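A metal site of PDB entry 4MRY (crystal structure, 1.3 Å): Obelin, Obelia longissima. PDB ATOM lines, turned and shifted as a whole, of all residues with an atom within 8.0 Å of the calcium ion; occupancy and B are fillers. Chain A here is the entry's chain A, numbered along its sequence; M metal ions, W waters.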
ATOM      1  N   PHE A  26      14.002 -18.454  17.573  1.00  0.00           N
ATOM      2  CA  PHE A  26      14.526 -18.405  16.209  1.00  0.00           C
ATOM      3  C   PHE A  26      14.014 -19.606  15.411  1.00  0.00           C
ATOM      4  O   PHE A  26      13.493 -19.437  14.302  1.00  0.00           O
ATOM      5  CB  PHE A  26      16.059 -18.383  16.281  1.00  0.00           C
ATOM      6  CG  PHE A  26      16.751 -18.379  14.929  1.00  0.00           C
ATOM      7  CD1 PHE A  26      17.043 -19.559  14.260  1.00  0.00           C
ATOM      8  CD2 PHE A  26      17.188 -17.189  14.371  1.00  0.00           C
ATOM      9  CE1 PHE A  26      17.694 -19.539  13.047  1.00  0.00           C
ATOM     10  CE2 PHE A  26      17.864 -17.171  13.158  1.00  0.00           C
ATOM     11  CZ  PHE A  26      18.116 -18.340  12.496  1.00  0.00           C
ATOM     12  N   ASP A  27      14.141 -20.809  15.961  1.00  0.00           N
ATOM     13  CA  ASP A  27      13.698 -22.016  15.264  1.00  0.00           C
ATOM     14  C   ASP A  27      12.195 -21.986  15.017  1.00  0.00           C
ATOM     15  O   ASP A  27      11.744 -22.383  13.942  1.00  0.00           O
ATOM     16  CB  ASP A  27      14.058 -23.262  16.071  1.00  0.00           C
ATOM     17  CG  ASP A  27      15.528 -23.579  16.014  1.00  0.00           C
ATOM     18  OD1 ASP A  27      16.262 -22.950  15.227  1.00  0.00           O
ATOM     19  OD2 ASP A  27      15.955 -24.488  16.773  1.00  0.00           O
ATOM     20  N   LEU A  29      10.175 -19.317  14.735  1.00  0.00           N
ATOM     21  CA  LEU A  29       9.832 -18.292  13.748  1.00  0.00           C
ATOM     22  C   LEU A  29      10.331 -18.609  12.347  1.00  0.00           C
ATOM     23  O   LEU A  29       9.822 -18.073  11.357  1.00  0.00           O
ATOM     24  CB  LEU A  29      10.378 -16.938  14.187  1.00  0.00           C
ATOM     25  CG  LEU A  29       9.852 -16.453  15.542  1.00  0.00           C
ATOM     26  CD1 LEU A  29      10.602 -15.210  15.996  1.00  0.00           C
ATOM     27  CD2 LEU A  29       8.353 -16.186  15.499  1.00  0.00           C
ATOM     28  N   ASP A  30      11.315 -19.484  12.273  1.00  0.00           N
ATOM     29  CA  ASP A  30      11.914 -19.922  11.008  1.00  0.00           C
ATOM     30  C   ASP A  30      10.945 -20.845  10.270  1.00  0.00           C
ATOM     31  O   ASP A  30      11.069 -22.067  10.317  1.00  0.00           O
ATOM     32  CB  ASP A  30      13.232 -20.629  11.308  1.00  0.00           C
ATOM     33  CG  ASP A  30      13.893 -21.225  10.065  1.00  0.00           C
ATOM     34  OD1 ASP A  30      13.544 -20.853   8.933  1.00  0.00           O
ATOM     35  OD2 ASP A  30      14.779 -22.068  10.286  1.00  0.00           O
ATOM     36  N   ILE A  31       9.980 -20.249   9.592  1.00  0.00           N
ATOM     37  CA  ILE A  31       8.871 -21.005   9.008  1.00  0.00           C
ATOM     38  C   ILE A  31       9.339 -22.144   8.111  1.00  0.00           C
ATOM     39  O   ILE A  31       8.881 -23.280   8.244  1.00  0.00           O
ATOM     40  CB  ILE A  31       7.924 -20.095   8.205  1.00  0.00           C
ATOM     41  CG1 ILE A  31       7.302 -19.034   9.100  1.00  0.00           C
ATOM     42  CG2 ILE A  31       6.846 -20.930   7.550  1.00  0.00           C
ATOM     43  CD1 ILE A  31       6.489 -17.982   8.331  1.00  0.00           C
ATOM     44  N   ASN A  32      10.244 -21.859   7.180  1.00  0.00           N
ATOM     45  CA  ASN A  32      10.675 -22.901   6.260  1.00  0.00           C
ATOM     46  C   ASN A  32      11.774 -23.826   6.833  1.00  0.00           C
ATOM     47  O   ASN A  32      12.204 -24.761   6.146  1.00  0.00           O
ATOM     48  CB  ASN A  32      11.012 -22.361   4.856  1.00  0.00           C
ATOM     49  CG  ASN A  32      12.232 -21.484   4.849  1.00  0.00           C
ATOM     50  OD1 ASN A  32      12.863 -21.303   5.869  1.00  0.00           O
ATOM     51  ND2 ASN A  32      12.582 -20.925   3.692  1.00  0.00           N
ATOM     52  N   GLY A  33      12.203 -23.594   8.064  1.00  0.00           N
ATOM     53  CA  GLY A  33      13.118 -24.497   8.761  1.00  0.00           C
ATOM     54  C   GLY A  33      14.534 -24.497   8.228  1.00  0.00           C
ATOM     55  O   GLY A  33      15.309 -25.399   8.539  1.00  0.00           O
ATOM     56  N   ASN A  34      14.905 -23.494   7.430  1.00  0.00           N
ATOM     57  CA  ASN A  34      16.203 -23.537   6.760  1.00  0.00           C
ATOM     58  C   ASN A  34      17.372 -22.989   7.571  1.00  0.00           C
ATOM     59  O   ASN A  34      18.498 -22.926   7.069  1.00  0.00           O
ATOM     60  CB  ASN A  34      16.132 -22.885   5.365  1.00  0.00           C
ATOM     61  CG  ASN A  34      16.164 -21.390   5.435  1.00  0.00           C
ATOM     62  OD1 ASN A  34      15.823 -20.800   6.439  1.00  0.00           O
ATOM     63  ND2 ASN A  34      16.601 -20.749   4.352  1.00  0.00           N
ATOM     64  N   GLY A  35      17.126 -22.588   8.821  1.00  0.00           N
ATOM     65  CA  GLY A  35      18.193 -22.090   9.674  1.00  0.00           C
ATOM     66  C   GLY A  35      18.591 -20.635   9.461  1.00  0.00           C
ATOM     67  O   GLY A  35      19.580 -20.161   9.987  1.00  0.00           O
ATOM     68  N   LYS A  36      17.784 -19.925   8.686  1.00  0.00           N
ATOM     69  CA  LYS A  36      17.988 -18.495   8.449  1.00  0.00           C
ATOM     70  C   LYS A  36      16.698 -17.799   8.748  1.00  0.00           C
ATOM     71  O   LYS A  36      15.631 -18.363   8.427  1.00  0.00           O
ATOM     72  CB  LYS A  36      18.363 -18.254   6.994  1.00  0.00           C
ATOM     73  CG  LYS A  36      19.629 -18.966   6.552  1.00  0.00           C
ATOM     74  CD  LYS A  36      20.844 -18.262   7.108  1.00  0.00           C
ATOM     75  CE  LYS A  36      22.106 -18.671   6.374  1.00  0.00           C
ATOM     76  NZ  LYS A  36      22.228 -20.142   6.325  1.00  0.00           N
ATOM     77  N   ILE A  37      16.633 -16.654   9.403  1.00  0.00           N
ATOM     78  CA  ILE A  37      15.366 -15.977   9.669  1.00  0.00           C
ATOM     79  C   ILE A  37      15.294 -14.718   8.802  1.00  0.00           C
ATOM     80  O   ILE A  37      16.322 -14.116   8.519  1.00  0.00           O
ATOM     81  CB  ILE A  37      15.221 -15.626  11.179  1.00  0.00           C
ATOM     82  CG1 ILE A  37      13.783 -15.246  11.519  1.00  0.00           C
ATOM     83  CG2 ILE A  37      16.174 -14.524  11.604  1.00  0.00           C
ATOM     84  CD1 ILE A  37      12.836 -16.405  11.460  1.00  0.00           C
ATOM     85  N   THR A  38      14.093 -14.351   8.350  1.00  0.00           N
ATOM     86  CA  THR A  38      13.878 -13.083   7.655  1.00  0.00           C
ATOM     87  C   THR A  38      12.861 -12.263   8.452  1.00  0.00           C
ATOM     88  O   THR A  38      12.070 -12.830   9.223  1.00  0.00           O
ATOM     89  CB  THR A  38      13.334 -13.277   6.236  1.00  0.00           C
ATOM     90  OG1 THR A  38      12.051 -13.916   6.324  1.00  0.00           O
ATOM     91  CG2 THR A  38      14.279 -14.135   5.393  1.00  0.00           C
ATOM     92  N   GLU A  41       9.395 -13.776   7.822  1.00  0.00           N
ATOM     93  CA  GLU A  41       8.995 -14.894   8.661  1.00  0.00           C
ATOM     94  C   GLU A  41       8.607 -14.410  10.042  1.00  0.00           C
ATOM     95  O   GLU A  41       7.626 -14.862  10.628  1.00  0.00           O
ATOM     96  CB  GLU A  41      10.125 -15.930   8.767  1.00  0.00           C
ATOM     97  CG  GLU A  41      10.278 -16.723   7.509  1.00  0.00           C
ATOM     98  CD  GLU A  41      11.414 -17.688   7.583  1.00  0.00           C
ATOM     99  OE1 GLU A  41      12.459 -17.321   8.189  1.00  0.00           O
ATOM    100  OE2 GLU A  41      11.267 -18.812   7.022  1.00  0.00           O
ATOM    101  N   GLU A  82      18.091 -12.892   4.724  1.00  0.00           N
ATOM    102  CA  GLU A  82      18.228 -14.111   5.509  1.00  0.00           C
ATOM    103  C   GLU A  82      19.387 -13.989   6.481  1.00  0.00           C
ATOM    104  O   GLU A  82      20.522 -13.703   6.072  1.00  0.00           O
ATOM    105  CB  GLU A  82      18.445 -15.319   4.610  1.00  0.00           C
ATOM    106  CG  GLU A  82      17.199 -15.800   3.923  1.00  0.00           C
ATOM    107  CD  GLU A  82      17.371 -17.191   3.375  1.00  0.00           C
ATOM    108  OE1 GLU A  82      18.351 -17.434   2.630  1.00  0.00           O
ATOM    109  OE2 GLU A  82      16.527 -18.051   3.699  1.00  0.00           O
ATOM    110  N   ILE A  83      19.105 -14.191   7.754  1.00  0.00           N
ATOM    111  CA  ILE A  83      20.091 -14.025   8.815  1.00  0.00           C
ATOM    112  C   ILE A  83      20.191 -15.290   9.670  1.00  0.00           C
ATOM    113  O   ILE A  83      19.171 -15.832  10.105  1.00  0.00           O
ATOM    114  CB  ILE A  83      19.749 -12.801   9.672  1.00  0.00           C
ATOM    115  CG1 ILE A  83      19.736 -11.574   8.756  1.00  0.00           C
ATOM    116  CG2 ILE A  83      20.734 -12.636  10.842  1.00  0.00           C
ATOM    117  CD1 ILE A  83      19.370 -10.298   9.406  1.00  0.00           C
HETATM  118 CA    CA M   1      13.811 -19.368   7.184  1.00  0.00          CA
HETATM  119  O   HOH W   1      14.325 -17.985   5.038  1.00  0.00           O
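The side-chain carboxylate (OD1) of Asp 30 lies close to the backbone NH (N) of Gly 33 (3.2 Å). The backbone NH (N) of Gly 35 lies within hydrogen-bond range of the side-chain carboxylate (OD2) of Asp 30 (2.8 Å). ND2 of Asn 34 sits at hydrogen-bond distance from OE2 of Glu 82. The backbone NH (N) of Ile 31 lies close to the side-chain carboxylate (OE2) of Glu 41. The backbone NH (N) of Glu 41 lies within hydrogen-bond range of the side-chain hydroxyl (OG1) of Thr 38 (3.1 Å).
Of the 15 residues printed, 5 come within 4 Å of the calcium ion.
The calcium ion is bound by the side-chain carboxylate (OD1) of Asp 30, the backbone carbonyl oxygen (O) of Lys 36, the side-chain amide oxygen (OD1) of Asn 32, the side-chain amide oxygen (OD1) of Asn 34, water W1, the side-chain carboxylate (OE2) of Glu 41 and the side-chain carboxylate (OE1) of Glu 41. The calcium ion has seven donor atoms within binding distance.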
